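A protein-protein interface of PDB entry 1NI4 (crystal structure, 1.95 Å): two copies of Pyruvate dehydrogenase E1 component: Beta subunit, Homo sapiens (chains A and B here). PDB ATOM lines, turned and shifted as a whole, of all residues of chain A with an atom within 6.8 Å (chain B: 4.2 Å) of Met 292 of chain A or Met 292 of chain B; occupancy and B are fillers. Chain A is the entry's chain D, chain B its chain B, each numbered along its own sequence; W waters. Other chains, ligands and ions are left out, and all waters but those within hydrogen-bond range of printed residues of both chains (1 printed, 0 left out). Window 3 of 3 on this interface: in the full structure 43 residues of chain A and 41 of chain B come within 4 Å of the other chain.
Of the 10 printed residues of chain B, 6 touch a printed residue of chain A. Along chain B the printed residues that touch a printed residue of chain A span positions 289 to 304. Of the 19 printed residues of chain A, 6 touch a printed residue of chain B. Hydrophobic or aromatic side chains of chain A within 4 Å of the printed part of chain B: Met 292, Phe 297, Pro 303 and Ala 304. Among the printed residues, 11 pairs touch across the chains. Among the printed residues, no Asp or Glu carboxylate lies within 4 Å of a Lys or Arg side-chain nitrogen of the other chain.
N of Ala 304 of chain B is in hydrogen-bond range of SD of Met 292 of chain A. SD of Met 292 of chain B sits at hydrogen-bond distance from N of Ala 304 of chain A, at 3.8 Å.
Of the printed residues of chain B, Cys 288 of chain A touches Met 292 (3.3 Å). Ala 289 of chain A touches none of the printed residues of chain B. Of chain B, only Met 292, Phe 297, Pro 303 and Ala 304 come within 4 Å of Met 292 of chain A. Of the printed residues of chain B, Pro 303 of chain A touches Met 292 (3.3 Å) and Phe 297 (3.7 Å). Met 292 of chain B touches just these residues of chain A: Cys 288, Met 292, Pro 303 and Ala 304. Of the printed residues of chain A, Glu 293 of chain B touches Ala 304. Of the printed residues of chain A, Phe 297 of chain B touches Met 292 and Pro 303. Of the printed residues of chain A, Ala 304 of chain B touches Met 292 (3.6 Å). The nearest residue of chain A that does not touch Met 292 of chain B is Leu 300 of chain A (4.5 Å). The nearest printed residue of chain A that does not touch Glu 293 of chain B is Val 305 of chain A (4.002 Å).
O of Ile 291 of chain A lies close to N of Phe 297 of chain A (3.4 Å).
Water W1 lies within hydrogen-bond range of the backbone carbonyl oxygen of Ala 304 of chain B and the backbone carbonyl oxygen of Met 292 of chain A.
Among the printed residues, merely in contact across the chains: Ala 285 of chain A with Ala 289 of chain B, Cys 288 of chain A with Met 292 of chain B, Met 292 of chain A with Met 292 of chain B, Met 292 of chain A with Phe 297 of chain B, Met 292 of chain A with Pro 303 of chain B, Phe 297 of chain A with Pro 303 of chain B, Pro 303 of chain A with Met 292 of chain B, Pro 303 of chain A with Phe 297 of chain B and Ala 304 of chain A with Glu 293 of chain B.
Cys 288 of chain A touches Met 292 of chain B, but with the chains exchanged Met 292 of chain A does not touch Cys 288 of chain B (4.5 Å). Met 292 of chain A touches Phe 297 of chain B, but with the chains exchanged Phe 297 of chain A does not touch Met 292 of chain B (4.9 Å). Phe 297 of chain A touches Pro 303 of chain B, and with the chains exchanged Pro 303 of chain A touches Phe 297 of chain B. Ala 304 of chain A touches Glu 293 of chain B, but with the chains exchanged Glu 293 of chain A does not touch Ala 304 of chain B (4.2 Å). 10 positions are printed for both chains.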
ATOM      1  N   GLU A 262      13.531  -9.856 -32.604  1.00  0.00           N
ATOM      2  CA  GLU A 262      12.975 -10.655 -33.688  1.00  0.00           C
ATOM      3  C   GLU A 262      13.220  -9.992 -35.038  1.00  0.00           C
ATOM      4  O   GLU A 262      13.554 -10.665 -36.014  1.00  0.00           O
ATOM      5  CB  GLU A 262      11.474 -10.890 -33.467  1.00  0.00           C
ATOM      6  CG  GLU A 262      11.176 -11.702 -32.206  1.00  0.00           C
ATOM      7  CD  GLU A 262       9.689 -11.950 -31.981  1.00  0.00           C
ATOM      8  OE1 GLU A 262       8.893 -10.999 -32.155  1.00  0.00           O
ATOM      9  OE2 GLU A 262       9.317 -13.092 -31.612  1.00  0.00           O
ATOM     10  N   LEU A 271      21.194 -16.277 -34.102  1.00  0.00           N
ATOM     11  CA  LEU A 271      21.065 -15.607 -32.814  1.00  0.00           C
ATOM     12  C   LEU A 271      21.934 -16.192 -31.717  1.00  0.00           C
ATOM     13  O   LEU A 271      22.043 -17.409 -31.571  1.00  0.00           O
ATOM     14  CB  LEU A 271      19.600 -15.625 -32.354  1.00  0.00           C
ATOM     15  CG  LEU A 271      19.325 -15.088 -30.942  1.00  0.00           C
ATOM     16  CD1 LEU A 271      19.651 -13.607 -30.873  1.00  0.00           C
ATOM     17  CD2 LEU A 271      17.863 -15.316 -30.583  1.00  0.00           C
ATOM     18  N   ALA A 285      17.564 -18.197 -21.644  1.00  0.00           N
ATOM     19  CA  ALA A 285      16.544 -19.213 -21.868  1.00  0.00           C
ATOM     20  C   ALA A 285      15.233 -18.582 -22.317  1.00  0.00           C
ATOM     21  O   ALA A 285      14.572 -19.083 -23.232  1.00  0.00           O
ATOM     22  CB  ALA A 285      16.324 -20.029 -20.591  1.00  0.00           C
ATOM     23  N   ILE A 287      14.766 -15.673 -23.829  1.00  0.00           N
ATOM     24  CA  ILE A 287      14.887 -15.133 -25.179  1.00  0.00           C
ATOM     25  C   ILE A 287      14.692 -16.247 -26.210  1.00  0.00           C
ATOM     26  O   ILE A 287      13.889 -16.116 -27.134  1.00  0.00           O
ATOM     27  CB  ILE A 287      16.263 -14.467 -25.390  1.00  0.00           C
ATOM     28  CG1 ILE A 287      16.381 -13.241 -24.482  1.00  0.00           C
ATOM     29  CG2 ILE A 287      16.425 -14.056 -26.851  1.00  0.00           C
ATOM     30  CD1 ILE A 287      17.708 -12.515 -24.589  1.00  0.00           C
ATOM     31  N   CYS A 288      15.421 -17.346 -26.041  1.00  0.00           N
ATOM     32  CA  CYS A 288      15.313 -18.481 -26.949  1.00  0.00           C
ATOM     33  C   CYS A 288      13.880 -19.014 -27.029  1.00  0.00           C
ATOM     34  O   CYS A 288      13.387 -19.320 -28.111  1.00  0.00           O
ATOM     35  CB  CYS A 288      16.265 -19.600 -26.510  1.00  0.00           C
ATOM     36  SG  CYS A 288      18.024 -19.165 -26.675  1.00  0.00           S
ATOM     37  N   ALA A 289      13.205 -19.122 -25.891  1.00  0.00           N
ATOM     38  CA  ALA A 289      11.838 -19.619 -25.896  1.00  0.00           C
ATOM     39  C   ALA A 289      10.915 -18.660 -26.647  1.00  0.00           C
ATOM     40  O   ALA A 289      10.062 -19.091 -27.420  1.00  0.00           O
ATOM     41  CB  ALA A 289      11.340 -19.826 -24.460  1.00  0.00           C
ATOM     42  N   ARG A 290      11.087 -17.363 -26.413  1.00  0.00           N
ATOM     43  CA  ARG A 290      10.273 -16.352 -27.079  1.00  0.00           C
ATOM     44  C   ARG A 290      10.502 -16.432 -28.590  1.00  0.00           C
ATOM     45  O   ARG A 290       9.574 -16.284 -29.383  1.00  0.00           O
ATOM     46  CB  ARG A 290      10.649 -14.950 -26.580  1.00  0.00           C
ATOM     47  CG  ARG A 290      10.287 -14.665 -25.130  1.00  0.00           C
ATOM     48  CD  ARG A 290       8.830 -14.277 -24.983  1.00  0.00           C
ATOM     49  NE  ARG A 290       8.688 -12.872 -24.600  1.00  0.00           N
ATOM     50  CZ  ARG A 290       8.962 -12.387 -23.389  1.00  0.00           C
ATOM     51  NH1 ARG A 290       9.392 -13.185 -22.424  1.00  0.00           N
ATOM     52  NH2 ARG A 290       8.811 -11.093 -23.144  1.00  0.00           N
ATOM     53  N   ILE A 291      11.751 -16.657 -28.981  1.00  0.00           N
ATOM     54  CA  ILE A 291      12.088 -16.756 -30.389  1.00  0.00           C
ATOM     55  C   ILE A 291      11.386 -17.941 -31.035  1.00  0.00           C
ATOM     56  O   ILE A 291      10.836 -17.826 -32.133  1.00  0.00           O
ATOM     57  CB  ILE A 291      13.612 -16.902 -30.583  1.00  0.00           C
ATOM     58  CG1 ILE A 291      14.290 -15.551 -30.344  1.00  0.00           C
ATOM     59  CG2 ILE A 291      13.920 -17.420 -31.971  1.00  0.00           C
ATOM     60  CD1 ILE A 291      13.761 -14.438 -31.232  1.00  0.00           C
ATOM     61  N   MET A 292      11.398 -19.075 -30.342  1.00  0.00           N
ATOM     62  CA  MET A 292      10.771 -20.288 -30.850  1.00  0.00           C
ATOM     63  C   MET A 292       9.245 -20.202 -30.915  1.00  0.00           C
ATOM     64  O   MET A 292       8.617 -20.882 -31.723  1.00  0.00           O
ATOM     65  CB  MET A 292      11.190 -21.486 -29.999  1.00  0.00           C
ATOM     66  CG  MET A 292      10.740 -22.817 -30.574  1.00  0.00           C
ATOM     67  SD  MET A 292      11.711 -24.316 -29.841  1.00  0.00           S
ATOM     68  CE  MET A 292      13.182 -24.339 -31.092  1.00  0.00           C
ATOM     69  N   GLU A 293       8.649 -19.367 -30.071  1.00  0.00           N
ATOM     70  CA  GLU A 293       7.195 -19.208 -30.066  1.00  0.00           C
ATOM     71  C   GLU A 293       6.722 -18.130 -31.039  1.00  0.00           C
ATOM     72  O   GLU A 293       5.571 -18.150 -31.470  1.00  0.00           O
ATOM     73  CB  GLU A 293       6.687 -18.835 -28.668  1.00  0.00           C
ATOM     74  CG  GLU A 293       6.845 -19.895 -27.604  1.00  0.00           C
ATOM     75  CD  GLU A 293       6.173 -19.489 -26.301  1.00  0.00           C
ATOM     76  OE1 GLU A 293       6.513 -18.406 -25.769  1.00  0.00           O
ATOM     77  OE2 GLU A 293       5.304 -20.250 -25.816  1.00  0.00           O
ATOM     78  N   GLY A 294       7.602 -17.190 -31.373  1.00  0.00           N
ATOM     79  CA  GLY A 294       7.223 -16.104 -32.265  1.00  0.00           C
ATOM     80  C   GLY A 294       7.423 -16.324 -33.755  1.00  0.00           C
ATOM     81  O   GLY A 294       7.778 -17.418 -34.192  1.00  0.00           O
ATOM     82  N   PRO A 295       7.195 -15.280 -34.570  1.00  0.00           N
ATOM     83  CA  PRO A 295       7.342 -15.332 -36.030  1.00  0.00           C
ATOM     84  C   PRO A 295       8.780 -15.363 -36.551  1.00  0.00           C
ATOM     85  O   PRO A 295       9.002 -15.577 -37.743  1.00  0.00           O
ATOM     86  CB  PRO A 295       6.591 -14.088 -36.495  1.00  0.00           C
ATOM     87  CG  PRO A 295       6.853 -13.114 -35.379  1.00  0.00           C
ATOM     88  CD  PRO A 295       6.649 -13.975 -34.144  1.00  0.00           C
ATOM     89  N   ALA A 296       9.754 -15.165 -35.670  1.00  0.00           N
ATOM     90  CA  ALA A 296      11.153 -15.172 -36.088  1.00  0.00           C
ATOM     91  C   ALA A 296      11.763 -16.575 -36.146  1.00  0.00           C
ATOM     92  O   ALA A 296      12.837 -16.769 -36.723  1.00  0.00           O
ATOM     93  CB  ALA A 296      11.977 -14.289 -35.156  1.00  0.00           C
ATOM     94  N   PHE A 297      11.084 -17.553 -35.551  1.00  0.00           N
ATOM     95  CA  PHE A 297      11.601 -18.917 -35.545  1.00  0.00           C
ATOM     96  C   PHE A 297      11.930 -19.450 -36.944  1.00  0.00           C
ATOM     97  O   PHE A 297      12.971 -20.076 -37.142  1.00  0.00           O
ATOM     98  CB  PHE A 297      10.612 -19.859 -34.869  1.00  0.00           C
ATOM     99  CG  PHE A 297      11.064 -21.289 -34.860  1.00  0.00           C
ATOM    100  CD1 PHE A 297      12.208 -21.661 -34.161  1.00  0.00           C
ATOM    101  CD2 PHE A 297      10.367 -22.258 -35.574  1.00  0.00           C
ATOM    102  CE1 PHE A 297      12.651 -22.978 -34.173  1.00  0.00           C
ATOM    103  CE2 PHE A 297      10.801 -23.579 -35.595  1.00  0.00           C
ATOM    104  CZ  PHE A 297      11.948 -23.941 -34.892  1.00  0.00           C
ATOM    105  N   LEU A 300      15.265 -18.455 -38.684  1.00  0.00           N
ATOM    106  CA  LEU A 300      16.483 -19.022 -38.120  1.00  0.00           C
ATOM    107  C   LEU A 300      17.102 -20.021 -39.096  1.00  0.00           C
ATOM    108  O   LEU A 300      16.391 -20.830 -39.684  1.00  0.00           O
ATOM    109  CB  LEU A 300      16.132 -19.724 -36.810  1.00  0.00           C
ATOM    110  CG  LEU A 300      16.782 -19.314 -35.487  1.00  0.00           C
ATOM    111  CD1 LEU A 300      17.111 -17.832 -35.444  1.00  0.00           C
ATOM    112  CD2 LEU A 300      15.830 -19.696 -34.365  1.00  0.00           C
ATOM    113  N   ALA A 302      19.909 -21.620 -38.038  1.00  0.00           N
ATOM    114  CA  ALA A 302      20.677 -22.415 -37.090  1.00  0.00           C
ATOM    115  C   ALA A 302      20.075 -22.223 -35.703  1.00  0.00           C
ATOM    116  O   ALA A 302      19.443 -21.203 -35.422  1.00  0.00           O
ATOM    117  CB  ALA A 302      22.132 -21.976 -37.093  1.00  0.00           C
ATOM    118  N   PRO A 303      20.251 -23.206 -34.816  1.00  0.00           N
ATOM    119  CA  PRO A 303      19.686 -23.057 -33.474  1.00  0.00           C
ATOM    120  C   PRO A 303      20.353 -21.931 -32.689  1.00  0.00           C
ATOM    121  O   PRO A 303      21.564 -21.736 -32.776  1.00  0.00           O
ATOM    122  CB  PRO A 303      19.923 -24.430 -32.850  1.00  0.00           C
ATOM    123  CG  PRO A 303      21.202 -24.881 -33.519  1.00  0.00           C
ATOM    124  CD  PRO A 303      20.960 -24.489 -34.959  1.00  0.00           C
ATOM    125  N   ALA A 304      19.558 -21.187 -31.929  1.00  0.00           N
ATOM    126  CA  ALA A 304      20.084 -20.090 -31.121  1.00  0.00           C
ATOM    127  C   ALA A 304      20.982 -20.671 -30.032  1.00  0.00           C
ATOM    128  O   ALA A 304      20.652 -21.700 -29.450  1.00  0.00           O
ATOM    129  CB  ALA A 304      18.930 -19.317 -30.491  1.00  0.00           C
ATOM    130  N   VAL A 305      22.116 -20.029 -29.760  1.00  0.00           N
ATOM    131  CA  VAL A 305      23.020 -20.525 -28.727  1.00  0.00           C
ATOM    132  C   VAL A 305      23.156 -19.527 -27.576  1.00  0.00           C
ATOM    133  O   VAL A 305      23.034 -18.316 -27.774  1.00  0.00           O
ATOM    134  CB  VAL A 305      24.423 -20.857 -29.306  1.00  0.00           C
ATOM    135  CG1 VAL A 305      24.269 -21.690 -30.561  1.00  0.00           C
ATOM    136  CG2 VAL A 305      25.202 -19.594 -29.585  1.00  0.00           C
ATOM    137  N   CYS B 288      12.779 -25.502 -23.367  1.00  0.00           N
ATOM    138  CA  CYS B 288      12.812 -25.107 -24.771  1.00  0.00           C
ATOM    139  C   CYS B 288      14.217 -24.678 -25.218  1.00  0.00           C
ATOM    140  O   CYS B 288      14.584 -24.856 -26.376  1.00  0.00           O
ATOM    141  CB  CYS B 288      11.820 -23.966 -25.023  1.00  0.00           C
ATOM    142  SG  CYS B 288      10.076 -24.410 -24.737  1.00  0.00           S
ATOM    143  N   ALA B 289      14.998 -24.109 -24.304  1.00  0.00           N
ATOM    144  CA  ALA B 289      16.356 -23.681 -24.626  1.00  0.00           C
ATOM    145  C   ALA B 289      17.279 -24.895 -24.720  1.00  0.00           C
ATOM    146  O   ALA B 289      18.178 -24.933 -25.559  1.00  0.00           O
ATOM    147  CB  ALA B 289      16.873 -22.707 -23.566  1.00  0.00           C
ATOM    148  N   ARG B 290      17.058 -25.880 -23.852  1.00  0.00           N
ATOM    149  CA  ARG B 290      17.858 -27.100 -23.851  1.00  0.00           C
ATOM    150  C   ARG B 290      17.578 -27.918 -25.114  1.00  0.00           C
ATOM    151  O   ARG B 290      18.497 -28.434 -25.747  1.00  0.00           O
ATOM    152  CB  ARG B 290      17.542 -27.938 -22.614  1.00  0.00           C
ATOM    153  CG  ARG B 290      17.880 -27.238 -21.313  1.00  0.00           C
ATOM    154  CD  ARG B 290      19.376 -27.210 -21.091  1.00  0.00           C
ATOM    155  NE  ARG B 290      19.851 -28.484 -20.562  1.00  0.00           N
ATOM    156  CZ  ARG B 290      19.766 -28.839 -19.283  1.00  0.00           C
ATOM    157  NH1 ARG B 290      19.229 -28.012 -18.392  1.00  0.00           N
ATOM    158  NH2 ARG B 290      20.209 -30.027 -18.896  1.00  0.00           N
ATOM    159  N   ILE B 291      16.308 -28.029 -25.479  1.00  0.00           N
ATOM    160  CA  ILE B 291      15.945 -28.771 -26.674  1.00  0.00           C
ATOM    161  C   ILE B 291      16.581 -28.127 -27.899  1.00  0.00           C
ATOM    162  O   ILE B 291      17.061 -28.822 -28.796  1.00  0.00           O
ATOM    163  CB  ILE B 291      14.412 -28.818 -26.870  1.00  0.00           C
ATOM    164  CG1 ILE B 291      13.802 -29.855 -25.932  1.00  0.00           C
ATOM    165  CG2 ILE B 291      14.072 -29.168 -28.316  1.00  0.00           C
ATOM    166  CD1 ILE B 291      14.285 -31.284 -26.204  1.00  0.00           C
ATOM    167  N   MET B 292      16.598 -26.798 -27.926  1.00  0.00           N
ATOM    168  CA  MET B 292      17.163 -26.076 -29.055  1.00  0.00           C
ATOM    169  C   MET B 292      18.668 -26.245 -29.168  1.00  0.00           C
ATOM    170  O   MET B 292      19.209 -26.289 -30.271  1.00  0.00           O
ATOM    171  CB  MET B 292      16.805 -24.592 -28.966  1.00  0.00           C
ATOM    172  CG  MET B 292      17.416 -23.734 -30.066  1.00  0.00           C
ATOM    173  SD  MET B 292      16.158 -22.469 -30.838  1.00  0.00           S
ATOM    174  CE  MET B 292      15.770 -21.414 -29.259  1.00  0.00           C
ATOM    175  N   GLU B 293      19.347 -26.352 -28.032  1.00  0.00           N
ATOM    176  CA  GLU B 293      20.796 -26.514 -28.036  1.00  0.00           C
ATOM    177  C   GLU B 293      21.209 -27.979 -28.108  1.00  0.00           C
ATOM    178  O   GLU B 293      22.372 -28.288 -28.361  1.00  0.00           O
ATOM    179  CB  GLU B 293      21.411 -25.889 -26.774  1.00  0.00           C
ATOM    180  CG  GLU B 293      21.364 -24.365 -26.720  1.00  0.00           C
ATOM    181  CD  GLU B 293      22.028 -23.804 -25.466  1.00  0.00           C
ATOM    182  OE1 GLU B 293      21.574 -24.154 -24.353  1.00  0.00           O
ATOM    183  OE2 GLU B 293      23.002 -23.020 -25.598  1.00  0.00           O
ATOM    184  N   GLY B 294      20.253 -28.876 -27.895  1.00  0.00           N
ATOM    185  CA  GLY B 294      20.563 -30.296 -27.898  1.00  0.00           C
ATOM    186  C   GLY B 294      20.507 -31.022 -29.226  1.00  0.00           C
ATOM    187  O   GLY B 294      20.272 -30.412 -30.267  1.00  0.00           O
ATOM    188  N   PHE B 297      17.090 -31.222 -31.482  1.00  0.00           N
ATOM    189  CA  PHE B 297      16.593 -30.075 -32.240  1.00  0.00           C
ATOM    190  C   PHE B 297      16.316 -30.400 -33.702  1.00  0.00           C
ATOM    191  O   PHE B 297      15.342 -29.916 -34.270  1.00  0.00           O
ATOM    192  CB  PHE B 297      17.564 -28.891 -32.169  1.00  0.00           C
ATOM    193  CG  PHE B 297      17.069 -27.662 -32.886  1.00  0.00           C
ATOM    194  CD1 PHE B 297      15.937 -26.987 -32.437  1.00  0.00           C
ATOM    195  CD2 PHE B 297      17.716 -27.195 -34.029  1.00  0.00           C
ATOM    196  CE1 PHE B 297      15.452 -25.862 -33.116  1.00  0.00           C
ATOM    197  CE2 PHE B 297      17.243 -26.074 -34.714  1.00  0.00           C
ATOM    198  CZ  PHE B 297      16.108 -25.406 -34.257  1.00  0.00           C
ATOM    199  N   PRO B 303       7.914 -25.922 -33.770  1.00  0.00           N
ATOM    200  CA  PRO B 303       8.484 -25.329 -32.556  1.00  0.00           C
ATOM    201  C   PRO B 303       7.775 -25.803 -31.286  1.00  0.00           C
ATOM    202  O   PRO B 303       6.595 -26.152 -31.312  1.00  0.00           O
ATOM    203  CB  PRO B 303       8.323 -23.831 -32.799  1.00  0.00           C
ATOM    204  CG  PRO B 303       7.072 -23.760 -33.611  1.00  0.00           C
ATOM    205  CD  PRO B 303       7.251 -24.900 -34.598  1.00  0.00           C
ATOM    206  N   ALA B 304       8.506 -25.840 -30.178  1.00  0.00           N
ATOM    207  CA  ALA B 304       7.918 -26.259 -28.912  1.00  0.00           C
ATOM    208  C   ALA B 304       7.044 -25.117 -28.402  1.00  0.00           C
ATOM    209  O   ALA B 304       7.338 -23.952 -28.652  1.00  0.00           O
ATOM    210  CB  ALA B 304       9.013 -26.574 -27.907  1.00  0.00           C
HETATM  211  O   HOH W   1       6.033 -22.543 -30.256  1.00  0.00           O
